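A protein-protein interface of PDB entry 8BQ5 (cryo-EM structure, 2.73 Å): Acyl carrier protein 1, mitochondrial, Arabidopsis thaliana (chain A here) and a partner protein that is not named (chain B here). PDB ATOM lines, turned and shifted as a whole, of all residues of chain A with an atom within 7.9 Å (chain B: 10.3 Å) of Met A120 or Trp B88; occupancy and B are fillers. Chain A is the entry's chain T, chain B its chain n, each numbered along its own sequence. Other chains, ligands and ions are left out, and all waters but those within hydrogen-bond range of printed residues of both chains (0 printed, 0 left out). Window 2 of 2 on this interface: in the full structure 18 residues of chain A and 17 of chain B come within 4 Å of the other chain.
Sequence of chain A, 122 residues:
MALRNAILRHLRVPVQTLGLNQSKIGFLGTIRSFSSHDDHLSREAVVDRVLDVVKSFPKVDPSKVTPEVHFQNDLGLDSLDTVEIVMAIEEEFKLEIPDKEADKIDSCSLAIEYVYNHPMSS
Asp A39 touches none of the printed residues of chain B. Of the printed residues of chain B, Glu A90 touches Arg B25. Of the printed residues of chain B, Glu A96 touches Ile B85 (3.7 Å), Val B86 (3.0 Å), Trp B88 (3.9 Å) and Ala B89 (3.6 Å). Of chain B, only Trp B88 comes within 4 Å of Met A120. No residue of chain B comes within 4 Å of Ser A121. Of the printed residues of chain A, Arg B25 touches Glu A90 and Ile A97. Printed residues of chain A within 4 Å of Tyr B84: Lys A94. Ala B89 touches one residue of chain A. Phe B95 touches none of the printed residues of chain A. The nearest residue of chain B that does not touch Met A120 is Lys B94 (5.5 Å). The nearest printed residue of chain A that does not touch Trp B88 is Leu A95 (4.001 Å). The nearest printed residue of chain A that does not touch Arg B25 is Pro A98 (4.4 Å).
Of the 18 printed residues of chain B, 6 touch a printed residue of chain A. Printed residues of chain B that touch a printed residue of chain A: Arg B25, Tyr B84, Ile B85, Val B86, Trp B88 and Ala B89. Along chain B the printed residues that touch a printed residue of chain A span positions 25 to 89. Among the printed residues, Asp or Glu carboxylates within 4 Å of a Lys or Arg side-chain nitrogen of the other chain: Glu A90 with Arg B25 (2.7 Å).
OE1 of Glu A90 sits close to N of Ile A97, at 3.1 Å. The backbone carbonyl oxygen of Glu A90 is in hydrogen-bond range of the backbone NH of Leu A95 (3.1 Å). The backbone NH of Met A120 lies within hydrogen-bond range of a ring nitrogen (ND1) of His A118, 3.1 Å away.
Among the printed residues, pairs that only touch across the chains: Lys A94 with Tyr B84 (3.7 Å), Lys A94 with Val B86 (3.9 Å), Lys A94 with Trp B88 (3.5 Å), Glu A96 with Ile B85 (3.7 Å), Glu A96 with Trp B88 (3.9 Å), Glu A96 with Ala B89 (3.6 Å), His A118 with Trp B88 (3.5 Å) and Met A120 with Trp B88 (3.8 Å).
O of Ile A97 sits at hydrogen-bond distance from NH2 of Arg B25, 2.8 Å away. The side-chain carboxylate (OE1) of Glu A96 sits at hydrogen-bond distance from the backbone NH (N) of Val B86. OE2 of Glu A90 lies within salt-bridge range of NH2 of Arg B25, 2.7 Å away.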
ATOM      1  N   ASP A  39       8.375  -4.284  22.933  1.00  0.00           N
ATOM      2  CA  ASP A  39       9.286  -4.466  24.057  1.00  0.00           C
ATOM      3  C   ASP A  39      10.729  -4.537  23.579  1.00  0.00           C
ATOM      4  O   ASP A  39      10.992  -4.587  22.379  1.00  0.00           O
ATOM      5  CB  ASP A  39       8.928  -5.733  24.838  1.00  0.00           C
ATOM      6  CG  ASP A  39       8.900  -5.506  26.337  1.00  0.00           C
ATOM      7  OD1 ASP A  39       9.578  -4.568  26.805  1.00  0.00           O
ATOM      8  OD2 ASP A  39       8.202  -6.261  27.044  1.00  0.00           O
ATOM      9  N   HIS A  40      11.666  -4.531  24.523  1.00  0.00           N
ATOM     10  CA  HIS A  40      13.054  -4.770  24.176  1.00  0.00           C
ATOM     11  C   HIS A  40      13.256  -6.246  23.839  1.00  0.00           C
ATOM     12  O   HIS A  40      12.444  -7.109  24.185  1.00  0.00           O
ATOM     13  CB  HIS A  40      13.977  -4.354  25.320  1.00  0.00           C
ATOM     14  CG  HIS A  40      15.215  -3.638  24.871  1.00  0.00           C
ATOM     15  ND1 HIS A  40      15.241  -2.282  24.627  1.00  0.00           N
ATOM     16  CD2 HIS A  40      16.467  -4.089  24.623  1.00  0.00           C
ATOM     17  CE1 HIS A  40      16.457  -1.928  24.251  1.00  0.00           C
ATOM     18  NE2 HIS A  40      17.220  -3.005  24.238  1.00  0.00           N
ATOM     19  N   LEU A  41      14.353  -6.531  23.149  1.00  0.00           N
ATOM     20  CA  LEU A  41      14.686  -7.891  22.757  1.00  0.00           C
ATOM     21  C   LEU A  41      15.832  -8.400  23.619  1.00  0.00           C
ATOM     22  O   LEU A  41      16.897  -7.778  23.687  1.00  0.00           O
ATOM     23  CB  LEU A  41      15.045  -7.953  21.271  1.00  0.00           C
ATOM     24  CG  LEU A  41      15.489  -9.303  20.710  1.00  0.00           C
ATOM     25  CD1 LEU A  41      14.362 -10.318  20.820  1.00  0.00           C
ATOM     26  CD2 LEU A  41      15.905  -9.150  19.263  1.00  0.00           C
ATOM     27  N   GLU A  90      22.141  -7.066   9.641  1.00  0.00           N
ATOM     28  CA  GLU A  90      21.289  -5.893   9.477  1.00  0.00           C
ATOM     29  C   GLU A  90      19.893  -6.291   9.025  1.00  0.00           C
ATOM     30  O   GLU A  90      18.891  -5.807   9.563  1.00  0.00           O
ATOM     31  CB  GLU A  90      21.900  -4.932   8.457  1.00  0.00           C
ATOM     32  CG  GLU A  90      23.369  -4.644   8.656  1.00  0.00           C
ATOM     33  CD  GLU A  90      23.611  -3.295   9.277  1.00  0.00           C
ATOM     34  OE1 GLU A  90      22.762  -2.855  10.078  1.00  0.00           O
ATOM     35  OE2 GLU A  90      24.644  -2.673   8.959  1.00  0.00           O
ATOM     36  N   PHE A  93      17.552  -7.932  11.867  1.00  0.00           N
ATOM     37  CA  PHE A  93      16.969  -7.042  12.860  1.00  0.00           C
ATOM     38  C   PHE A  93      16.448  -5.738  12.268  1.00  0.00           C
ATOM     39  O   PHE A  93      15.886  -4.923  13.008  1.00  0.00           O
ATOM     40  CB  PHE A  93      17.997  -6.731  13.955  1.00  0.00           C
ATOM     41  CG  PHE A  93      18.422  -7.933  14.755  1.00  0.00           C
ATOM     42  CD1 PHE A  93      17.688  -8.346  15.854  1.00  0.00           C
ATOM     43  CD2 PHE A  93      19.559  -8.645  14.410  1.00  0.00           C
ATOM     44  CE1 PHE A  93      18.077  -9.446  16.591  1.00  0.00           C
ATOM     45  CE2 PHE A  93      19.953  -9.749  15.144  1.00  0.00           C
ATOM     46  CZ  PHE A  93      19.211 -10.150  16.235  1.00  0.00           C
ATOM     47  N   LYS A  94      16.611  -5.523  10.959  1.00  0.00           N
ATOM     48  CA  LYS A  94      16.212  -4.286  10.280  1.00  0.00           C
ATOM     49  C   LYS A  94      16.893  -3.067  10.906  1.00  0.00           C
ATOM     50  O   LYS A  94      16.248  -2.113  11.346  1.00  0.00           O
ATOM     51  CB  LYS A  94      14.689  -4.118  10.273  1.00  0.00           C
ATOM     52  CG  LYS A  94      14.160  -3.194   9.185  1.00  0.00           C
ATOM     53  CD  LYS A  94      12.716  -2.788   9.451  1.00  0.00           C
ATOM     54  CE  LYS A  94      12.198  -1.832   8.386  1.00  0.00           C
ATOM     55  NZ  LYS A  94      10.773  -1.459   8.617  1.00  0.00           N
ATOM     56  N   LEU A  95      18.220  -3.109  10.925  1.00  0.00           N
ATOM     57  CA  LEU A  95      19.022  -2.024  11.465  1.00  0.00           C
ATOM     58  C   LEU A  95      19.872  -1.400  10.369  1.00  0.00           C
ATOM     59  O   LEU A  95      20.230  -2.046   9.381  1.00  0.00           O
ATOM     60  CB  LEU A  95      19.929  -2.502  12.605  1.00  0.00           C
ATOM     61  CG  LEU A  95      19.276  -3.293  13.733  1.00  0.00           C
ATOM     62  CD1 LEU A  95      20.326  -4.109  14.467  1.00  0.00           C
ATOM     63  CD2 LEU A  95      18.539  -2.363  14.681  1.00  0.00           C
ATOM     64  N   GLU A  96      20.184  -0.123  10.558  1.00  0.00           N
ATOM     65  CA  GLU A  96      21.050   0.631   9.657  1.00  0.00           C
ATOM     66  C   GLU A  96      22.276   1.058  10.457  1.00  0.00           C
ATOM     67  O   GLU A  96      22.285   2.120  11.083  1.00  0.00           O
ATOM     68  CB  GLU A  96      20.325   1.830   9.059  1.00  0.00           C
ATOM     69  CG  GLU A  96      21.100   2.520   7.951  1.00  0.00           C
ATOM     70  CD  GLU A  96      20.199   3.111   6.887  1.00  0.00           C
ATOM     71  OE1 GLU A  96      19.219   2.443   6.497  1.00  0.00           O
ATOM     72  OE2 GLU A  96      20.476   4.243   6.438  1.00  0.00           O
ATOM     73  N   ILE A  97      23.302   0.220  10.448  1.00  0.00           N
ATOM     74  CA  ILE A  97      24.570   0.582  11.082  1.00  0.00           C
ATOM     75  C   ILE A  97      25.299   1.574  10.180  1.00  0.00           C
ATOM     76  O   ILE A  97      25.289   1.400   8.951  1.00  0.00           O
ATOM     77  CB  ILE A  97      25.420  -0.660  11.330  1.00  0.00           C
ATOM     78  CG1 ILE A  97      24.654  -1.663  12.188  1.00  0.00           C
ATOM     79  CG2 ILE A  97      26.717  -0.289  12.020  1.00  0.00           C
ATOM     80  CD1 ILE A  97      25.302  -3.022  12.256  1.00  0.00           C
ATOM     81  N   PRO A  98      25.912   2.619  10.732  1.00  0.00           N
ATOM     82  CA  PRO A  98      26.769   3.479   9.911  1.00  0.00           C
ATOM     83  C   PRO A  98      27.977   2.710   9.400  1.00  0.00           C
ATOM     84  O   PRO A  98      28.386   1.697   9.972  1.00  0.00           O
ATOM     85  CB  PRO A  98      27.179   4.596  10.874  1.00  0.00           C
ATOM     86  CG  PRO A  98      26.092   4.622  11.896  1.00  0.00           C
ATOM     87  CD  PRO A  98      25.673   3.192  12.067  1.00  0.00           C
ATOM     88  N   VAL A 115      24.139  -5.184  18.542  1.00  0.00           N
ATOM     89  CA  VAL A 115      22.677  -5.337  18.294  1.00  0.00           C
ATOM     90  C   VAL A 115      21.912  -5.217  19.618  1.00  0.00           C
ATOM     91  O   VAL A 115      20.852  -4.567  19.618  1.00  0.00           O
ATOM     92  CB  VAL A 115      22.368  -6.660  17.566  1.00  0.00           C
ATOM     93  CG1 VAL A 115      20.875  -6.923  17.479  1.00  0.00           C
ATOM     94  CG2 VAL A 115      22.994  -6.691  16.182  1.00  0.00           C
ATOM     95  N   TYR A 116      22.420  -5.817  20.699  1.00  0.00           N
ATOM     96  CA  TYR A 116      21.659  -5.817  21.976  1.00  0.00           C
ATOM     97  C   TYR A 116      21.540  -4.383  22.504  1.00  0.00           C
ATOM     98  O   TYR A 116      20.430  -3.978  22.894  1.00  0.00           O
ATOM     99  CB  TYR A 116      22.287  -6.773  22.993  1.00  0.00           C
ATOM    100  CG  TYR A 116      21.567  -6.820  24.316  1.00  0.00           C
ATOM    101  CD1 TYR A 116      20.199  -7.019  24.375  1.00  0.00           C
ATOM    102  CD2 TYR A 116      22.249  -6.657  25.509  1.00  0.00           C
ATOM    103  CE1 TYR A 116      19.525  -7.054  25.583  1.00  0.00           C
ATOM    104  CE2 TYR A 116      21.592  -6.697  26.728  1.00  0.00           C
ATOM    105  CZ  TYR A 116      20.224  -6.896  26.766  1.00  0.00           C
ATOM    106  OH  TYR A 116      19.563  -6.935  27.959  1.00  0.00           O
ATOM    107  N   ASN A 117      22.640  -3.633  22.484  1.00  0.00           N
ATOM    108  CA  ASN A 117      22.635  -2.267  22.993  1.00  0.00           C
ATOM    109  C   ASN A 117      21.813  -1.314  22.136  1.00  0.00           C
ATOM    110  O   ASN A 117      21.536  -0.194  22.577  1.00  0.00           O
ATOM    111  CB  ASN A 117      24.065  -1.733  23.108  1.00  0.00           C
ATOM    112  CG  ASN A 117      24.883  -2.477  24.140  1.00  0.00           C
ATOM    113  OD1 ASN A 117      24.351  -2.956  25.141  1.00  0.00           O
ATOM    114  ND2 ASN A 117      26.187  -2.565  23.911  1.00  0.00           N
ATOM    115  N   HIS A 118      21.426  -1.722  20.937  1.00  0.00           N
ATOM    116  CA  HIS A 118      20.649  -0.852  20.061  1.00  0.00           C
ATOM    117  C   HIS A 118      19.205  -0.772  20.538  1.00  0.00           C
ATOM    118  O   HIS A 118      18.550  -1.812  20.682  1.00  0.00           O
ATOM    119  CB  HIS A 118      20.706  -1.360  18.625  1.00  0.00           C
ATOM    120  CG  HIS A 118      20.398  -0.309  17.604  1.00  0.00           C
ATOM    121  ND1 HIS A 118      19.288   0.504  17.684  1.00  0.00           N
ATOM    122  CD2 HIS A 118      21.056   0.065  16.482  1.00  0.00           C
ATOM    123  CE1 HIS A 118      19.274   1.331  16.657  1.00  0.00           C
ATOM    124  NE2 HIS A 118      20.335   1.085  15.911  1.00  0.00           N
ATOM    125  N   PRO A 119      18.669   0.426  20.789  1.00  0.00           N
ATOM    126  CA  PRO A 119      17.289   0.526  21.288  1.00  0.00           C
ATOM    127  C   PRO A 119      16.227   0.132  20.275  1.00  0.00           C
ATOM    128  O   PRO A 119      15.077  -0.086  20.673  1.00  0.00           O
ATOM    129  CB  PRO A 119      17.161   2.006  21.668  1.00  0.00           C
ATOM    130  CG  PRO A 119      18.167   2.700  20.807  1.00  0.00           C
ATOM    131  CD  PRO A 119      19.314   1.744  20.666  1.00  0.00           C
ATOM    132  N   MET A 120      16.558   0.049  18.988  1.00  0.00           N
ATOM    133  CA  MET A 120      15.567  -0.232  17.959  1.00  0.00           C
ATOM    134  C   MET A 120      15.628  -1.663  17.441  1.00  0.00           C
ATOM    135  O   MET A 120      14.883  -2.004  16.518  1.00  0.00           O
ATOM    136  CB  MET A 120      15.719   0.753  16.798  1.00  0.00           C
ATOM    137  CG  MET A 120      15.182   2.153  17.081  1.00  0.00           C
ATOM    138  SD  MET A 120      13.442   2.400  16.654  1.00  0.00           S
ATOM    139  CE  MET A 120      12.603   1.689  18.070  1.00  0.00           C
ATOM    140  N   SER A 121      16.485  -2.507  18.007  1.00  0.00           N
ATOM    141  CA  SER A 121      16.573  -3.892  17.559  1.00  0.00           C
ATOM    142  C   SER A 121      15.310  -4.657  17.941  1.00  0.00           C
ATOM    143  O   SER A 121      14.786  -5.445  17.154  1.00  0.00           O
ATOM    144  CB  SER A 121      17.802  -4.584  18.148  1.00  0.00           C
ATOM    145  OG  SER A 121      17.512  -5.154  19.412  1.00  0.00           O
ATOM    146  N   ARG B  25      30.873  -2.681   1.035  1.00  0.00           N
ATOM    147  CA  ARG B  25      29.632  -2.583   1.796  1.00  0.00           C
ATOM    148  C   ARG B  25      28.627  -1.673   1.100  1.00  0.00           C
ATOM    149  O   ARG B  25      27.430  -1.979   1.054  1.00  0.00           O
ATOM    150  CB  ARG B  25      29.923  -2.087   3.213  1.00  0.00           C
ATOM    151  CG  ARG B  25      28.741  -1.429   3.914  1.00  0.00           C
ATOM    152  CD  ARG B  25      28.820  -1.622   5.423  1.00  0.00           C
ATOM    153  NE  ARG B  25      27.753  -0.928   6.135  1.00  0.00           N
ATOM    154  CZ  ARG B  25      26.707  -1.525   6.691  1.00  0.00           C
ATOM    155  NH1 ARG B  25      26.530  -2.833   6.605  1.00  0.00           N
ATOM    156  NH2 ARG B  25      25.812  -0.789   7.346  1.00  0.00           N
ATOM    157  N   LYS B  29      25.008  -2.681  -1.041  1.00  0.00           N
ATOM    158  CA  LYS B  29      23.706  -2.112  -0.707  1.00  0.00           C
ATOM    159  C   LYS B  29      23.094  -1.388  -1.897  1.00  0.00           C
ATOM    160  O   LYS B  29      21.869  -1.393  -2.061  1.00  0.00           O
ATOM    161  CB  LYS B  29      23.820  -1.163   0.483  1.00  0.00           C
ATOM    162  CG  LYS B  29      23.915  -1.858   1.828  1.00  0.00           C
ATOM    163  CD  LYS B  29      24.578  -0.957   2.853  1.00  0.00           C
ATOM    164  CE  LYS B  29      24.294  -1.429   4.266  1.00  0.00           C
ATOM    165  NZ  LYS B  29      23.513  -0.426   5.038  1.00  0.00           N
ATOM    166  N   TYR B  84      17.254   3.157  -0.622  1.00  0.00           N
ATOM    167  CA  TYR B  84      16.414   2.829   0.518  1.00  0.00           C
ATOM    168  C   TYR B  84      17.113   3.205   1.817  1.00  0.00           C
ATOM    169  O   TYR B  84      18.325   3.023   1.964  1.00  0.00           O
ATOM    170  CB  TYR B  84      16.071   1.340   0.518  1.00  0.00           C
ATOM    171  CG  TYR B  84      15.427   0.879   1.802  1.00  0.00           C
ATOM    172  CD1 TYR B  84      14.069   1.063   2.024  1.00  0.00           C
ATOM    173  CD2 TYR B  84      16.177   0.269   2.797  1.00  0.00           C
ATOM    174  CE1 TYR B  84      13.480   0.654   3.200  1.00  0.00           C
ATOM    175  CE2 TYR B  84      15.596  -0.143   3.974  1.00  0.00           C
ATOM    176  CZ  TYR B  84      14.249   0.050   4.172  1.00  0.00           C
ATOM    177  OH  TYR B  84      13.672  -0.366   5.347  1.00  0.00           O
ATOM    178  N   ILE B  85      16.342   3.733   2.765  1.00  0.00           N
ATOM    179  CA  ILE B  85      16.835   4.060   4.098  1.00  0.00           C
ATOM    180  C   ILE B  85      15.820   3.558   5.114  1.00  0.00           C
ATOM    181  O   ILE B  85      14.613   3.754   4.939  1.00  0.00           O
ATOM    182  CB  ILE B  85      17.074   5.574   4.265  1.00  0.00           C
ATOM    183  CG1 ILE B  85      18.303   6.013   3.473  1.00  0.00           C
ATOM    184  CG2 ILE B  85      17.262   5.935   5.729  1.00  0.00           C
ATOM    185  CD1 ILE B  85      18.321   7.488   3.153  1.00  0.00           C
ATOM    186  N   VAL B  86      16.309   2.901   6.163  1.00  0.00           N
ATOM    187  CA  VAL B  86      15.433   2.452   7.253  1.00  0.00           C
ATOM    188  C   VAL B  86      14.745   3.665   7.870  1.00  0.00           C
ATOM    189  O   VAL B  86      15.403   4.701   8.091  1.00  0.00           O
ATOM    190  CB  VAL B  86      16.249   1.673   8.302  1.00  0.00           C
ATOM    191  CG1 VAL B  86      15.384   1.245   9.472  1.00  0.00           C
ATOM    192  CG2 VAL B  86      16.891   0.455   7.659  1.00  0.00           C
ATOM    193  N   PRO B  87      13.439   3.603   8.160  1.00  0.00           N
ATOM    194  CA  PRO B  87      12.690   4.834   8.479  1.00  0.00           C
ATOM    195  C   PRO B  87      13.264   5.670   9.615  1.00  0.00           C
ATOM    196  O   PRO B  87      13.250   6.903   9.517  1.00  0.00           O
ATOM    197  CB  PRO B  87      11.296   4.302   8.833  1.00  0.00           C
ATOM    198  CG  PRO B  87      11.174   3.050   8.043  1.00  0.00           C
ATOM    199  CD  PRO B  87      12.545   2.441   8.011  1.00  0.00           C
ATOM    200  N   TRP B  88      13.762   5.057  10.683  1.00  0.00           N
ATOM    201  CA  TRP B  88      14.287   5.824  11.804  1.00  0.00           C
ATOM    202  C   TRP B  88      15.764   6.163  11.652  1.00  0.00           C
ATOM    203  O   TRP B  88      16.307   6.891  12.489  1.00  0.00           O
ATOM    204  CB  TRP B  88      14.054   5.069  13.116  1.00  0.00           C
ATOM    205  CG  TRP B  88      14.432   3.633  13.043  1.00  0.00           C
ATOM    206  CD1 TRP B  88      13.597   2.575  12.846  1.00  0.00           C
ATOM    207  CD2 TRP B  88      15.749   3.088  13.171  1.00  0.00           C
ATOM    208  NE1 TRP B  88      14.312   1.404  12.838  1.00  0.00           N
ATOM    209  CE2 TRP B  88      15.637   1.692  13.036  1.00  0.00           C
ATOM    210  CE3 TRP B  88      17.014   3.647  13.384  1.00  0.00           C
ATOM    211  CZ2 TRP B  88      16.739   0.845  13.107  1.00  0.00           C
ATOM    212  CZ3 TRP B  88      18.107   2.805  13.454  1.00  0.00           C
ATOM    213  CH2 TRP B  88      17.963   1.419  13.316  1.00  0.00           C
ATOM    214  N   ALA B  89      16.422   5.653  10.617  1.00  0.00           N
ATOM    215  CA  ALA B  89      17.793   6.023  10.316  1.00  0.00           C
ATOM    216  C   ALA B  89      17.843   7.434   9.743  1.00  0.00           C
ATOM    217  O   ALA B  89      16.842   7.939   9.230  1.00  0.00           O
ATOM    218  CB  ALA B  89      18.402   5.027   9.333  1.00  0.00           C
ATOM    219  N   PRO B  90      18.991   8.105   9.843  1.00  0.00           N
ATOM    220  CA  PRO B  90      19.099   9.467   9.299  1.00  0.00           C
ATOM    221  C   PRO B  90      18.734   9.508   7.823  1.00  0.00           C
ATOM    222  O   PRO B  90      19.181   8.679   7.028  1.00  0.00           O
ATOM    223  CB  PRO B  90      20.572   9.831   9.529  1.00  0.00           C
ATOM    224  CG  PRO B  90      21.225   8.610  10.127  1.00  0.00           C
ATOM    225  CD  PRO B  90      20.140   7.767  10.696  1.00  0.00           C
ATOM    226  N   GLY B  91      17.916  10.495   7.460  1.00  0.00           N
ATOM    227  CA  GLY B  91      17.365  10.585   6.128  1.00  0.00           C
ATOM    228  C   GLY B  91      16.134   9.738   5.896  1.00  0.00           C
ATOM    229  O   GLY B  91      15.570   9.784   4.795  1.00  0.00           O
ATOM    230  N   GLY B  92      15.702   8.959   6.890  1.00  0.00           N
ATOM    231  CA  GLY B  92      14.506   8.162   6.751  1.00  0.00           C
ATOM    232  C   GLY B  92      13.243   8.969   6.976  1.00  0.00           C
ATOM    233  O   GLY B  92      13.267  10.101   7.456  1.00  0.00           O
ATOM    234  N   SER B  93      12.110   8.354   6.625  1.00  0.00           N
ATOM    235  CA  SER B  93      10.834   9.057   6.700  1.00  0.00           C
ATOM    236  C   SER B  93      10.359   9.226   8.137  1.00  0.00           C
ATOM    237  O   SER B  93       9.526  10.097   8.412  1.00  0.00           O
ATOM    238  CB  SER B  93       9.778   8.316   5.882  1.00  0.00           C
ATOM    239  OG  SER B  93       9.548   7.018   6.399  1.00  0.00           O
ATOM    240  N   LYS B  94      10.857   8.408   9.059  1.00  0.00           N
ATOM    241  CA  LYS B  94      10.496   8.512  10.465  1.00  0.00           C
ATOM    242  C   LYS B  94      11.554   9.227  11.294  1.00  0.00           C
ATOM    243  O   LYS B  94      11.414   9.308  12.518  1.00  0.00           O
ATOM    244  CB  LYS B  94      10.233   7.115  11.043  1.00  0.00           C
ATOM    245  CG  LYS B  94       9.263   7.096  12.216  1.00  0.00           C
ATOM    246  CD  LYS B  94       9.573   5.959  13.174  1.00  0.00           C
ATOM    247  CE  LYS B  94       8.408   4.994  13.289  1.00  0.00           C
ATOM    248  NZ  LYS B  94       8.742   3.805  14.120  1.00  0.00           N
ATOM    249  N   PHE B  95      12.603   9.752  10.664  1.00  0.00           N
ATOM    250  CA  PHE B  95      13.693  10.370  11.408  1.00  0.00           C
ATOM    251  C   PHE B  95      13.237  11.666  12.069  1.00  0.00           C
ATOM    252  O   PHE B  95      12.526  12.468  11.460  1.00  0.00           O
ATOM    253  CB  PHE B  95      14.882  10.641  10.487  1.00  0.00           C
ATOM    254  CG  PHE B  95      16.161  10.922  11.222  1.00  0.00           C
ATOM    255  CD1 PHE B  95      16.560  10.117  12.274  1.00  0.00           C
ATOM    256  CD2 PHE B  95      16.960  11.996  10.865  1.00  0.00           C
ATOM    257  CE1 PHE B  95      17.734  10.373  12.956  1.00  0.00           C
ATOM    258  CE2 PHE B  95      18.137  12.258  11.545  1.00  0.00           C
ATOM    259  CZ  PHE B  95      18.524  11.446  12.592  1.00  0.00           C
ATOM    260  N   CYS B  96      13.655  11.863  13.322  1.00  0.00           N
ATOM    261  CA  CYS B  96      13.359  13.067  14.101  1.00  0.00           C
ATOM    262  C   CYS B  96      11.862  13.270  14.319  1.00  0.00           C
ATOM    263  O   CYS B  96      11.414  14.393  14.561  1.00  0.00           O
ATOM    264  CB  CYS B  96      13.970  14.319  13.460  1.00  0.00           C
ATOM    265  SG  CYS B  96      15.752  14.244  13.181  1.00  0.00           S
ATOM    266  N   ARG B  97      11.075  12.201  14.242  1.00  0.00           N
ATOM    267  CA  ARG B  97       9.643  12.283  14.497  1.00  0.00           C
ATOM    268  C   ARG B  97       9.351  11.855  15.929  1.00  0.00           C
ATOM    269  O   ARG B  97       9.654  10.723  16.317  1.00  0.00           O
ATOM    270  CB  ARG B  97       8.856  11.411  13.521  1.00  0.00           C
ATOM    271  CG  ARG B  97       7.359  11.597  13.650  1.00  0.00           C
ATOM    272  CD  ARG B  97       6.586  10.407  13.124  1.00  0.00           C
ATOM    273  NE  ARG B  97       6.746  10.231  11.687  1.00  0.00           N
ATOM    274  CZ  ARG B  97       6.112   9.308  10.976  1.00  0.00           C
ATOM    275  NH1 ARG B  97       5.271   8.458  11.540  1.00  0.00           N
ATOM    276  NH2 ARG B  97       6.321   9.242   9.665  1.00  0.00           N
ATOM    277  N   ASN B  98       8.740  12.760  16.697  1.00  0.00           N
ATOM    278  CA  ASN B  98       8.494  12.590  18.125  1.00  0.00           C
ATOM    279  C   ASN B  98       9.735  12.071  18.842  1.00  0.00           C
ATOM    280  O   ASN B  98       9.682  11.009  19.476  1.00  0.00           O
ATOM    281  CB  ASN B  98       7.314  11.645  18.364  1.00  0.00           C
ATOM    282  CG  ASN B  98       6.028  12.156  17.753  1.00  0.00           C
ATOM    283  OD1 ASN B  98       5.663  13.318  17.929  1.00  0.00           O
ATOM    284  ND2 ASN B  98       5.330  11.288  17.033  1.00  0.00           N
ATOM    285  N   PRO B  99      10.865  12.771  18.765  1.00  0.00           N
ATOM    286  CA  PRO B  99      12.059  12.300  19.468  1.00  0.00           C
ATOM    287  C   PRO B  99      11.934  12.530  20.964  1.00  0.00           C
ATOM    288  O   PRO B  99      11.160  13.371  21.425  1.00  0.00           O
ATOM    289  CB  PRO B  99      13.178  13.147  18.863  1.00  0.00           C
ATOM    290  CG  PRO B  99      12.509  14.418  18.500  1.00  0.00           C
ATOM    291  CD  PRO B  99      11.095  14.074  18.114  1.00  0.00           C
